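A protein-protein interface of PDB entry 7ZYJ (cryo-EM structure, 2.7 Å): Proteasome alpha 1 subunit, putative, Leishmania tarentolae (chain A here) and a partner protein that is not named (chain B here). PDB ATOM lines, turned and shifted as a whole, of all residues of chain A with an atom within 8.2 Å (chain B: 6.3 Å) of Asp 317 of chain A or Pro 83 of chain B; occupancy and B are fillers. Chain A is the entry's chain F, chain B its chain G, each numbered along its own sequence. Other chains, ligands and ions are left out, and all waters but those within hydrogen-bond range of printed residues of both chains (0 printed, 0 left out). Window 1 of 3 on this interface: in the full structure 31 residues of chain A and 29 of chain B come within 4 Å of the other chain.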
ATOM      1  N   LEU A 183     -14.239 -10.152 -11.336  1.00  0.00           N
ATOM      2  CA  LEU A 183     -15.663 -10.061 -11.029  1.00  0.00           C
ATOM      3  C   LEU A 183     -16.003  -8.578 -10.927  1.00  0.00           C
ATOM      4  O   LEU A 183     -15.667  -7.921  -9.937  1.00  0.00           O
ATOM      5  CB  LEU A 183     -15.996 -10.812  -9.747  1.00  0.00           C
ATOM      6  CG  LEU A 183     -15.746 -12.321  -9.756  1.00  0.00           C
ATOM      7  CD1 LEU A 183     -15.780 -12.876  -8.342  1.00  0.00           C
ATOM      8  CD2 LEU A 183     -16.766 -13.025 -10.635  1.00  0.00           C
ATOM      9  N   ILE A 186     -18.439  -6.965  -7.982  1.00  0.00           N
ATOM     10  CA  ILE A 186     -17.763  -6.711  -6.715  1.00  0.00           C
ATOM     11  C   ILE A 186     -16.877  -5.475  -6.814  1.00  0.00           C
ATOM     12  O   ILE A 186     -16.791  -4.683  -5.869  1.00  0.00           O
ATOM     13  CB  ILE A 186     -16.975  -7.956  -6.263  1.00  0.00           C
ATOM     14  CG1 ILE A 186     -17.925  -9.131  -5.996  1.00  0.00           C
ATOM     15  CG2 ILE A 186     -16.142  -7.644  -5.041  1.00  0.00           C
ATOM     16  CD1 ILE A 186     -18.228 -10.006  -7.187  1.00  0.00           C
ATOM     17  N   ASN A 190     -17.015  -2.119  -4.561  1.00  0.00           N
ATOM     18  CA  ASN A 190     -15.864  -1.436  -3.973  1.00  0.00           C
ATOM     19  C   ASN A 190     -15.858   0.040  -4.347  1.00  0.00           C
ATOM     20  O   ASN A 190     -15.544   0.901  -3.517  1.00  0.00           O
ATOM     21  CB  ASN A 190     -14.554  -2.098  -4.408  1.00  0.00           C
ATOM     22  CG  ASN A 190     -14.420  -3.526  -3.913  1.00  0.00           C
ATOM     23  OD1 ASN A 190     -14.395  -4.469  -4.701  1.00  0.00           O
ATOM     24  ND2 ASN A 190     -14.322  -3.688  -2.600  1.00  0.00           N
ATOM     25  N   ALA A 274     -14.733 -11.292  13.023  1.00  0.00           N
ATOM     26  CA  ALA A 274     -14.259 -10.933  11.692  1.00  0.00           C
ATOM     27  C   ALA A 274     -14.476 -12.074  10.710  1.00  0.00           C
ATOM     28  O   ALA A 274     -14.870 -11.848   9.558  1.00  0.00           O
ATOM     29  CB  ALA A 274     -12.783 -10.541  11.748  1.00  0.00           C
ATOM     30  N   ILE A 277     -18.187 -12.019   9.789  1.00  0.00           N
ATOM     31  CA  ILE A 277     -18.502 -10.960   8.827  1.00  0.00           C
ATOM     32  C   ILE A 277     -17.999 -11.332   7.439  1.00  0.00           C
ATOM     33  O   ILE A 277     -18.682 -11.099   6.434  1.00  0.00           O
ATOM     34  CB  ILE A 277     -17.939  -9.599   9.280  1.00  0.00           C
ATOM     35  CG1 ILE A 277     -18.160  -9.376  10.771  1.00  0.00           C
ATOM     36  CG2 ILE A 277     -18.573  -8.472   8.484  1.00  0.00           C
ATOM     37  CD1 ILE A 277     -17.430  -8.173  11.321  1.00  0.00           C
ATOM     38  N   GLY A 278     -16.793 -11.896   7.357  1.00  0.00           N
ATOM     39  CA  GLY A 278     -16.281 -12.324   6.067  1.00  0.00           C
ATOM     40  C   GLY A 278     -17.144 -13.390   5.419  1.00  0.00           C
ATOM     41  O   GLY A 278     -17.422 -13.334   4.220  1.00  0.00           O
ATOM     42  N   GLU A 279     -17.581 -14.376   6.207  1.00  0.00           N
ATOM     43  CA  GLU A 279     -18.448 -15.421   5.673  1.00  0.00           C
ATOM     44  C   GLU A 279     -19.787 -14.847   5.221  1.00  0.00           C
ATOM     45  O   GLU A 279     -20.323 -15.245   4.179  1.00  0.00           O
ATOM     46  CB  GLU A 279     -18.654 -16.512   6.724  1.00  0.00           C
ATOM     47  CG  GLU A 279     -19.507 -17.683   6.263  1.00  0.00           C
ATOM     48  CD  GLU A 279     -18.860 -18.478   5.142  1.00  0.00           C
ATOM     49  OE1 GLU A 279     -17.614 -18.465   5.041  1.00  0.00           O
ATOM     50  OE2 GLU A 279     -19.597 -19.119   4.365  1.00  0.00           O
ATOM     51  N   HIS A 281     -20.328 -11.786   4.136  1.00  0.00           N
ATOM     52  CA  HIS A 281     -20.074 -11.088   2.879  1.00  0.00           C
ATOM     53  C   HIS A 281     -19.943 -12.071   1.724  1.00  0.00           C
ATOM     54  O   HIS A 281     -20.480 -11.845   0.634  1.00  0.00           O
ATOM     55  CB  HIS A 281     -18.811 -10.236   2.999  1.00  0.00           C
ATOM     56  CG  HIS A 281     -19.054  -8.864   3.544  1.00  0.00           C
ATOM     57  ND1 HIS A 281     -19.229  -8.617   4.888  1.00  0.00           N
ATOM     58  CD2 HIS A 281     -19.144  -7.663   2.926  1.00  0.00           C
ATOM     59  CE1 HIS A 281     -19.418  -7.324   5.074  1.00  0.00           C
ATOM     60  NE2 HIS A 281     -19.372  -6.722   3.900  1.00  0.00           N
ATOM     61  N   GLN A 282     -19.224 -13.175   1.946  1.00  0.00           N
ATOM     62  CA  GLN A 282     -19.017 -14.154   0.884  1.00  0.00           C
ATOM     63  C   GLN A 282     -20.315 -14.849   0.496  1.00  0.00           C
ATOM     64  O   GLN A 282     -20.459 -15.302  -0.644  1.00  0.00           O
ATOM     65  CB  GLN A 282     -17.972 -15.184   1.312  1.00  0.00           C
ATOM     66  CG  GLN A 282     -17.286 -15.890   0.154  1.00  0.00           C
ATOM     67  CD  GLN A 282     -18.072 -17.076  -0.362  1.00  0.00           C
ATOM     68  OE1 GLN A 282     -18.851 -17.686   0.371  1.00  0.00           O
ATOM     69  NE2 GLN A 282     -17.877 -17.408  -1.632  1.00  0.00           N
ATOM     70  N   ARG A 283     -21.268 -14.943   1.423  1.00  0.00           N
ATOM     71  CA  ARG A 283     -22.537 -15.593   1.116  1.00  0.00           C
ATOM     72  C   ARG A 283     -23.328 -14.869   0.034  1.00  0.00           C
ATOM     73  O   ARG A 283     -24.244 -15.468  -0.542  1.00  0.00           O
ATOM     74  CB  ARG A 283     -23.387 -15.703   2.382  1.00  0.00           C
ATOM     75  CG  ARG A 283     -24.321 -16.900   2.401  1.00  0.00           C
ATOM     76  CD  ARG A 283     -24.908 -17.117   3.785  1.00  0.00           C
ATOM     77  NE  ARG A 283     -23.877 -17.330   4.792  1.00  0.00           N
ATOM     78  CZ  ARG A 283     -23.740 -16.597   5.889  1.00  0.00           C
ATOM     79  NH1 ARG A 283     -24.556 -15.590   6.152  1.00  0.00           N
ATOM     80  NH2 ARG A 283     -22.762 -16.884   6.744  1.00  0.00           N
ATOM     81  N   ILE A 285     -21.950 -13.190  -2.774  1.00  0.00           N
ATOM     82  CA  ILE A 285     -21.140 -12.858  -3.941  1.00  0.00           C
ATOM     83  C   ILE A 285     -21.044 -14.044  -4.893  1.00  0.00           C
ATOM     84  O   ILE A 285     -20.283 -14.007  -5.866  1.00  0.00           O
ATOM     85  CB  ILE A 285     -19.733 -12.389  -3.530  1.00  0.00           C
ATOM     86  CG1 ILE A 285     -18.992 -13.505  -2.794  1.00  0.00           C
ATOM     87  CG2 ILE A 285     -19.817 -11.135  -2.674  1.00  0.00           C
ATOM     88  CD1 ILE A 285     -17.530 -13.217  -2.557  1.00  0.00           C
ATOM     89  N   GLN A 286     -21.812 -15.102  -4.630  1.00  0.00           N
ATOM     90  CA  GLN A 286     -21.753 -16.295  -5.462  1.00  0.00           C
ATOM     91  C   GLN A 286     -23.107 -16.801  -5.937  1.00  0.00           C
ATOM     92  O   GLN A 286     -23.141 -17.669  -6.815  1.00  0.00           O
ATOM     93  CB  GLN A 286     -21.032 -17.431  -4.721  1.00  0.00           C
ATOM     94  CG  GLN A 286     -20.244 -18.353  -5.634  1.00  0.00           C
ATOM     95  CD  GLN A 286     -19.252 -19.212  -4.882  1.00  0.00           C
ATOM     96  OE1 GLN A 286     -19.093 -19.079  -3.669  1.00  0.00           O
ATOM     97  NE2 GLN A 286     -18.575 -20.097  -5.601  1.00  0.00           N
ATOM     98  N   LEU A 297     -16.740  -1.626   6.301  1.00  0.00           N
ATOM     99  CA  LEU A 297     -16.864  -1.537   7.747  1.00  0.00           C
ATOM    100  C   LEU A 297     -15.496  -1.398   8.396  1.00  0.00           C
ATOM    101  O   LEU A 297     -14.507  -1.968   7.928  1.00  0.00           O
ATOM    102  CB  LEU A 297     -17.563  -2.771   8.319  1.00  0.00           C
ATOM    103  CG  LEU A 297     -19.024  -2.979   7.927  1.00  0.00           C
ATOM    104  CD1 LEU A 297     -19.529  -4.309   8.461  1.00  0.00           C
ATOM    105  CD2 LEU A 297     -19.878  -1.831   8.408  1.00  0.00           C
ATOM    106  N   TYR A 310     -10.481  -4.014  12.479  1.00  0.00           N
ATOM    107  CA  TYR A 310     -10.682  -4.741  11.236  1.00  0.00           C
ATOM    108  C   TYR A 310     -11.335  -3.849  10.190  1.00  0.00           C
ATOM    109  O   TYR A 310     -12.030  -2.881  10.508  1.00  0.00           O
ATOM    110  CB  TYR A 310     -11.546  -5.986  11.461  1.00  0.00           C
ATOM    111  CG  TYR A 310     -10.901  -7.035  12.331  1.00  0.00           C
ATOM    112  CD1 TYR A 310     -10.122  -8.040  11.776  1.00  0.00           C
ATOM    113  CD2 TYR A 310     -11.075  -7.026  13.707  1.00  0.00           C
ATOM    114  CE1 TYR A 310      -9.531  -9.002  12.566  1.00  0.00           C
ATOM    115  CE2 TYR A 310     -10.488  -7.986  14.505  1.00  0.00           C
ATOM    116  CZ  TYR A 310      -9.718  -8.971  13.930  1.00  0.00           C
ATOM    117  OH  TYR A 310      -9.131  -9.929  14.723  1.00  0.00           O
ATOM    118  N   GLN A 311     -11.094  -4.191   8.926  1.00  0.00           N
ATOM    119  CA  GLN A 311     -11.750  -3.538   7.800  1.00  0.00           C
ATOM    120  C   GLN A 311     -12.278  -4.611   6.864  1.00  0.00           C
ATOM    121  O   GLN A 311     -11.533  -5.515   6.472  1.00  0.00           O
ATOM    122  CB  GLN A 311     -10.796  -2.599   7.057  1.00  0.00           C
ATOM    123  CG  GLN A 311     -11.461  -1.829   5.928  1.00  0.00           C
ATOM    124  CD  GLN A 311     -10.519  -0.864   5.244  1.00  0.00           C
ATOM    125  OE1 GLN A 311      -9.340  -0.783   5.584  1.00  0.00           O
ATOM    126  NE2 GLN A 311     -11.035  -0.122   4.272  1.00  0.00           N
ATOM    127  N   THR A 312     -13.554  -4.514   6.506  1.00  0.00           N
ATOM    128  CA  THR A 312     -14.189  -5.459   5.601  1.00  0.00           C
ATOM    129  C   THR A 312     -14.554  -4.758   4.302  1.00  0.00           C
ATOM    130  O   THR A 312     -14.829  -3.554   4.289  1.00  0.00           O
ATOM    131  CB  THR A 312     -15.443  -6.079   6.223  1.00  0.00           C
ATOM    132  OG1 THR A 312     -16.406  -5.052   6.485  1.00  0.00           O
ATOM    133  CG2 THR A 312     -15.099  -6.785   7.525  1.00  0.00           C
ATOM    134  N   VAL A 313     -14.556  -5.517   3.217  1.00  0.00           N
ATOM    135  CA  VAL A 313     -14.829  -4.988   1.884  1.00  0.00           C
ATOM    136  C   VAL A 313     -15.924  -5.845   1.266  1.00  0.00           C
ATOM    137  O   VAL A 313     -16.180  -6.972   1.723  1.00  0.00           O
ATOM    138  CB  VAL A 313     -13.555  -4.951   1.010  1.00  0.00           C
ATOM    139  CG1 VAL A 313     -12.601  -3.884   1.516  1.00  0.00           C
ATOM    140  CG2 VAL A 313     -12.878  -6.305   1.012  1.00  0.00           C
ATOM    141  N   PRO A 314     -16.610  -5.335   0.238  1.00  0.00           N
ATOM    142  CA  PRO A 314     -17.686  -6.126  -0.382  1.00  0.00           C
ATOM    143  C   PRO A 314     -17.236  -7.478  -0.904  1.00  0.00           C
ATOM    144  O   PRO A 314     -18.052  -8.406  -0.958  1.00  0.00           O
ATOM    145  CB  PRO A 314     -18.165  -5.221  -1.522  1.00  0.00           C
ATOM    146  CG  PRO A 314     -17.856  -3.855  -1.061  1.00  0.00           C
ATOM    147  CD  PRO A 314     -16.590  -3.951  -0.265  1.00  0.00           C
ATOM    148  N   SER A 315     -15.971  -7.619  -1.303  1.00  0.00           N
ATOM    149  CA  SER A 315     -15.486  -8.909  -1.779  1.00  0.00           C
ATOM    150  C   SER A 315     -15.508  -9.972  -0.691  1.00  0.00           C
ATOM    151  O   SER A 315     -15.561 -11.163  -1.010  1.00  0.00           O
ATOM    152  CB  SER A 315     -14.070  -8.771  -2.339  1.00  0.00           C
ATOM    153  OG  SER A 315     -13.146  -8.443  -1.319  1.00  0.00           O
ATOM    154  N   GLY A 316     -15.481  -9.573   0.577  1.00  0.00           N
ATOM    155  CA  GLY A 316     -15.450 -10.501   1.688  1.00  0.00           C
ATOM    156  C   GLY A 316     -14.128 -10.551   2.417  1.00  0.00           C
ATOM    157  O   GLY A 316     -14.029 -11.245   3.437  1.00  0.00           O
ATOM    158  N   ASP A 317     -13.111  -9.847   1.930  1.00  0.00           N
ATOM    159  CA  ASP A 317     -11.827  -9.823   2.611  1.00  0.00           C
ATOM    160  C   ASP A 317     -11.912  -8.992   3.885  1.00  0.00           C
ATOM    161  O   ASP A 317     -12.518  -7.919   3.919  1.00  0.00           O
ATOM    162  CB  ASP A 317     -10.745  -9.259   1.691  1.00  0.00           C
ATOM    163  CG  ASP A 317     -10.388 -10.205   0.564  1.00  0.00           C
ATOM    164  OD1 ASP A 317     -11.051 -10.151  -0.493  1.00  0.00           O
ATOM    165  OD2 ASP A 317      -9.442 -11.003   0.734  1.00  0.00           O
ATOM    166  N   VAL A 318     -11.294  -9.504   4.945  1.00  0.00           N
ATOM    167  CA  VAL A 318     -11.216  -8.815   6.226  1.00  0.00           C
ATOM    168  C   VAL A 318      -9.746  -8.587   6.534  1.00  0.00           C
ATOM    169  O   VAL A 318      -8.957  -9.539   6.552  1.00  0.00           O
ATOM    170  CB  VAL A 318     -11.892  -9.609   7.357  1.00  0.00           C
ATOM    171  CG1 VAL A 318     -12.083  -8.725   8.578  1.00  0.00           C
ATOM    172  CG2 VAL A 318     -13.222 -10.174   6.888  1.00  0.00           C
ATOM    173  N   TYR A 319      -9.378  -7.333   6.775  1.00  0.00           N
ATOM    174  CA  TYR A 319      -7.992  -6.945   7.000  1.00  0.00           C
ATOM    175  C   TYR A 319      -7.811  -6.567   8.463  1.00  0.00           C
ATOM    176  O   TYR A 319      -8.560  -5.739   8.989  1.00  0.00           O
ATOM    177  CB  TYR A 319      -7.598  -5.776   6.098  1.00  0.00           C
ATOM    178  CG  TYR A 319      -7.800  -6.020   4.621  1.00  0.00           C
ATOM    179  CD1 TYR A 319      -9.026  -5.779   4.017  1.00  0.00           C
ATOM    180  CD2 TYR A 319      -6.759  -6.479   3.828  1.00  0.00           C
ATOM    181  CE1 TYR A 319      -9.212  -5.998   2.666  1.00  0.00           C
ATOM    182  CE2 TYR A 319      -6.935  -6.702   2.476  1.00  0.00           C
ATOM    183  CZ  TYR A 319      -8.163  -6.459   1.901  1.00  0.00           C
ATOM    184  OH  TYR A 319      -8.341  -6.679   0.555  1.00  0.00           O
ATOM    185  N   ASP A 320      -6.816  -7.168   9.109  1.00  0.00           N
ATOM    186  CA  ASP A 320      -6.443  -6.779  10.463  1.00  0.00           C
ATOM    187  C   ASP A 320      -5.453  -5.624  10.379  1.00  0.00           C
ATOM    188  O   ASP A 320      -4.356  -5.780   9.832  1.00  0.00           O
ATOM    189  CB  ASP A 320      -5.844  -7.966  11.212  1.00  0.00           C
ATOM    190  CG  ASP A 320      -5.797  -7.748  12.711  1.00  0.00           C
ATOM    191  OD1 ASP A 320      -6.268  -6.689  13.176  1.00  0.00           O
ATOM    192  OD2 ASP A 320      -5.292  -8.639  13.425  1.00  0.00           O
ATOM    193  N   ASN B  64      -5.040 -11.548   6.808  1.00  0.00           N
ATOM    194  CA  ASN B  64      -5.312 -12.267   5.563  1.00  0.00           C
ATOM    195  C   ASN B  64      -4.623 -13.628   5.548  1.00  0.00           C
ATOM    196  O   ASN B  64      -3.907 -13.973   4.605  1.00  0.00           O
ATOM    197  CB  ASN B  64      -4.902 -11.439   4.345  1.00  0.00           C
ATOM    198  CG  ASN B  64      -5.670 -10.140   4.242  1.00  0.00           C
ATOM    199  OD1 ASN B  64      -6.901 -10.130   4.239  1.00  0.00           O
ATOM    200  ND2 ASN B  64      -4.944  -9.031   4.168  1.00  0.00           N
ATOM    201  N   ARG B  66      -3.973 -17.263   4.801  1.00  0.00           N
ATOM    202  CA  ARG B  66      -4.390 -18.125   3.705  1.00  0.00           C
ATOM    203  C   ARG B  66      -4.289 -19.606   4.040  1.00  0.00           C
ATOM    204  O   ARG B  66      -4.790 -20.433   3.272  1.00  0.00           O
ATOM    205  CB  ARG B  66      -3.567 -17.822   2.446  1.00  0.00           C
ATOM    206  CG  ARG B  66      -3.641 -16.366   2.015  1.00  0.00           C
ATOM    207  CD  ARG B  66      -2.873 -16.115   0.730  1.00  0.00           C
ATOM    208  NE  ARG B  66      -3.662 -16.452  -0.448  1.00  0.00           N
ATOM    209  CZ  ARG B  66      -4.438 -15.597  -1.100  1.00  0.00           C
ATOM    210  NH1 ARG B  66      -4.555 -14.337  -0.713  1.00  0.00           N
ATOM    211  NH2 ARG B  66      -5.115 -16.015  -2.164  1.00  0.00           N
ATOM    212  N   ILE B  78      -4.963 -21.555   0.552  1.00  0.00           N
ATOM    213  CA  ILE B  78      -5.800 -20.961  -0.484  1.00  0.00           C
ATOM    214  C   ILE B  78      -4.903 -20.213  -1.457  1.00  0.00           C
ATOM    215  O   ILE B  78      -4.073 -19.393  -1.043  1.00  0.00           O
ATOM    216  CB  ILE B  78      -6.855 -20.021   0.118  1.00  0.00           C
ATOM    217  CG1 ILE B  78      -7.642 -20.741   1.213  1.00  0.00           C
ATOM    218  CG2 ILE B  78      -7.772 -19.492  -0.971  1.00  0.00           C
ATOM    219  CD1 ILE B  78      -8.323 -19.809   2.184  1.00  0.00           C
ATOM    220  N   GLY B  80      -5.702 -17.848  -4.510  1.00  0.00           N
ATOM    221  CA  GLY B  80      -6.738 -17.188  -5.279  1.00  0.00           C
ATOM    222  C   GLY B  80      -7.615 -16.276  -4.448  1.00  0.00           C
ATOM    223  O   GLY B  80      -7.137 -15.640  -3.504  1.00  0.00           O
ATOM    224  N   LEU B  81      -8.899 -16.200  -4.792  1.00  0.00           N
ATOM    225  CA  LEU B  81      -9.834 -15.354  -4.059  1.00  0.00           C
ATOM    226  C   LEU B  81      -9.992 -15.873  -2.636  1.00  0.00           C
ATOM    227  O   LEU B  81     -10.499 -16.978  -2.422  1.00  0.00           O
ATOM    228  CB  LEU B  81     -11.185 -15.314  -4.769  1.00  0.00           C
ATOM    229  CG  LEU B  81     -11.384 -14.257  -5.858  1.00  0.00           C
ATOM    230  CD1 LEU B  81     -10.543 -14.560  -7.088  1.00  0.00           C
ATOM    231  CD2 LEU B  81     -12.854 -14.151  -6.227  1.00  0.00           C
ATOM    232  N   LEU B  82      -9.555 -15.073  -1.666  1.00  0.00           N
ATOM    233  CA  LEU B  82      -9.518 -15.477  -0.266  1.00  0.00           C
ATOM    234  C   LEU B  82     -10.900 -15.794   0.308  1.00  0.00           C
ATOM    235  O   LEU B  82     -11.034 -16.798   1.013  1.00  0.00           O
ATOM    236  CB  LEU B  82      -8.822 -14.405   0.577  1.00  0.00           C
ATOM    237  CG  LEU B  82      -8.248 -14.879   1.913  1.00  0.00           C
ATOM    238  CD1 LEU B  82      -7.436 -16.150   1.725  1.00  0.00           C
ATOM    239  CD2 LEU B  82      -7.400 -13.791   2.551  1.00  0.00           C
ATOM    240  N   PRO B  83     -11.939 -14.973   0.081  1.00  0.00           N
ATOM    241  CA  PRO B  83     -13.268 -15.344   0.613  1.00  0.00           C
ATOM    242  C   PRO B  83     -13.799 -16.667   0.078  1.00  0.00           C
ATOM    243  O   PRO B  83     -14.422 -17.437   0.828  1.00  0.00           O
ATOM    244  CB  PRO B  83     -14.157 -14.165   0.189  1.00  0.00           C
ATOM    245  CG  PRO B  83     -13.370 -13.412  -0.829  1.00  0.00           C
ATOM    246  CD  PRO B  83     -11.949 -13.608  -0.469  1.00  0.00           C
ATOM    247  N   ASP B  84     -13.571 -16.958  -1.204  1.00  0.00           N
ATOM    248  CA  ASP B  84     -13.958 -18.257  -1.742  1.00  0.00           C
ATOM    249  C   ASP B  84     -13.192 -19.375  -1.052  1.00  0.00           C
ATOM    250  O   ASP B  84     -13.749 -20.442  -0.760  1.00  0.00           O
ATOM    251  CB  ASP B  84     -13.725 -18.291  -3.251  1.00  0.00           C
ATOM    252  CG  ASP B  84     -14.748 -17.476  -4.017  1.00  0.00           C
ATOM    253  OD1 ASP B  84     -15.806 -17.152  -3.438  1.00  0.00           O
ATOM    254  OD2 ASP B  84     -14.495 -17.160  -5.197  1.00  0.00           O
ATOM    255  N   GLY B  85     -11.907 -19.146  -0.780  1.00  0.00           N
ATOM    256  CA  GLY B  85     -11.139 -20.116  -0.024  1.00  0.00           C
ATOM    257  C   GLY B  85     -11.670 -20.309   1.381  1.00  0.00           C
ATOM    258  O   GLY B  85     -11.639 -21.416   1.914  1.00  0.00           O
ATOM    259  N   ARG B  86     -12.158 -19.235   2.004  1.00  0.00           N
ATOM    260  CA  ARG B  86     -12.757 -19.357   3.329  1.00  0.00           C
ATOM    261  C   ARG B  86     -14.026 -20.196   3.280  1.00  0.00           C
ATOM    262  O   ARG B  86     -14.275 -21.010   4.176  1.00  0.00           O
ATOM    263  CB  ARG B  86     -13.051 -17.974   3.909  1.00  0.00           C
ATOM    264  CG  ARG B  86     -11.828 -17.090   4.061  1.00  0.00           C
ATOM    265  CD  ARG B  86     -10.765 -17.766   4.907  1.00  0.00           C
ATOM    266  NE  ARG B  86     -11.198 -17.946   6.288  1.00  0.00           N
ATOM    267  CZ  ARG B  86     -11.134 -17.007   7.221  1.00  0.00           C
ATOM    268  NH1 ARG B  86     -10.650 -15.804   6.959  1.00  0.00           N
ATOM    269  NH2 ARG B  86     -11.563 -17.282   8.449  1.00  0.00           N
ATOM    270  N   ALA B  87     -14.843 -20.008   2.242  1.00  0.00           N
ATOM    271  CA  ALA B  87     -16.025 -20.851   2.078  1.00  0.00           C
ATOM    272  C   ALA B  87     -15.636 -22.315   1.892  1.00  0.00           C
ATOM    273  O   ALA B  87     -16.256 -23.216   2.478  1.00  0.00           O
ATOM    274  CB  ALA B  87     -16.860 -20.363   0.896  1.00  0.00           C
ATOM    275  N   ILE B  88     -14.607 -22.569   1.081  1.00  0.00           N
ATOM    276  CA  ILE B  88     -14.149 -23.938   0.862  1.00  0.00           C
ATOM    277  C   ILE B  88     -13.603 -24.534   2.155  1.00  0.00           C
ATOM    278  O   ILE B  88     -13.807 -25.717   2.448  1.00  0.00           O
ATOM    279  CB  ILE B  88     -13.107 -23.975  -0.271  1.00  0.00           C
ATOM    280  CG1 ILE B  88     -13.775 -23.659  -1.608  1.00  0.00           C
ATOM    281  CG2 ILE B  88     -12.415 -25.326  -0.332  1.00  0.00           C
ATOM    282  CD1 ILE B  88     -12.809 -23.554  -2.758  1.00  0.00           C
ATOM    283  N   CYS B 134     -10.454 -19.898  -6.589  1.00  0.00           N
ATOM    284  CA  CYS B 134      -9.282 -20.254  -5.809  1.00  0.00           C
ATOM    285  C   CYS B 134      -8.992 -21.737  -5.972  1.00  0.00           C
ATOM    286  O   CYS B 134      -9.895 -22.540  -6.220  1.00  0.00           O
ATOM    287  CB  CYS B 134      -9.467 -19.917  -4.326  1.00  0.00           C
ATOM    288  SG  CYS B 134     -10.971 -20.598  -3.602  1.00  0.00           S
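OD1 of Asp 84 of chain B sits at hydrogen-bond distance from NE2 of Gln 282 of chain A (2.8 Å). The side-chain amide oxygen (OD1) of Asn 64 of chain B sits close to the backbone carbonyl oxygen (O) of Val 318 of chain A, 3.2 Å away.
OD1 of Asp 317 of chain A lies within hydrogen-bond range of OG of Ser 315 of chain A, at 2.8 Å. The side-chain amide oxygen (OE1) of Gln 286 of chain A sits at hydrogen-bond distance from the side-chain amide nitrogen (NE2) of Gln 282 of chain A (2.9 Å). O of Gln 311 of chain A is in hydrogen-bond range of N of Tyr 319 of chain A (2.8 Å).
Of the printed residues of chain B, Gln 282 of chain A touches Pro 83, Asp 84 and Ala 87. Ile 285 of chain A touches none of the printed residues of chain B. Asp 317 of chain A touches two residues of chain B. Of the printed residues of chain B, Tyr 319 of chain A touches Asn 64. Printed residues of chain A within 4 Å of Asn 64 of chain B: Val 318 (3.2 Å) and Tyr 319 (3.2 Å). Arg 66 of chain B touches none of the printed residues of chain A. Of chain A, only Gln 282, Ser 315 and Asp 317 come within 4 Å of Pro 83 of chain B. Printed residues of chain A within 4 Å of Asp 84 of chain B: Gln 282 (2.8 Å) and Gln 286 (3.8 Å). The nearest printed residue of chain A that does not touch Leu 82 of chain B is Val 318 of chain A (6.0 Å).
Hydrophobic or aromatic side chains of chain B that line the printed part of chain A: Leu 81, Leu 82, Pro 83 and Ala 87. Hydrophobic or aromatic side chains of chain A within 4 Å of the printed part of chain B: Leu 183 and Tyr 319. Among the printed residues, 10 pairs touch across the chains. Among the printed residues, no Asp or Glu carboxylate lies within 4 Å of a Lys or Arg side-chain nitrogen of the other chain.
Among the printed residues, merely in contact across the chains: Ser 315 of chain A with Pro 83 of chain B (3.1 Å), Tyr 319 of chain A with Asn 64 of chain B (3.2 Å), Gln 282 of chain A with Pro 83 of chain B (3.3 Å), Gln 282 of chain A with Ala 87 of chain B (3.4 Å), Asp 317 of chain A with Leu 82 of chain B (3.5 Å), Asp 317 of chain A with Pro 83 of chain B (3.6 Å), Gln 286 of chain A with Asp 84 of chain B (3.8 Å) and Leu 183 of chain A with Leu 81 of chain B (3.8 Å).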
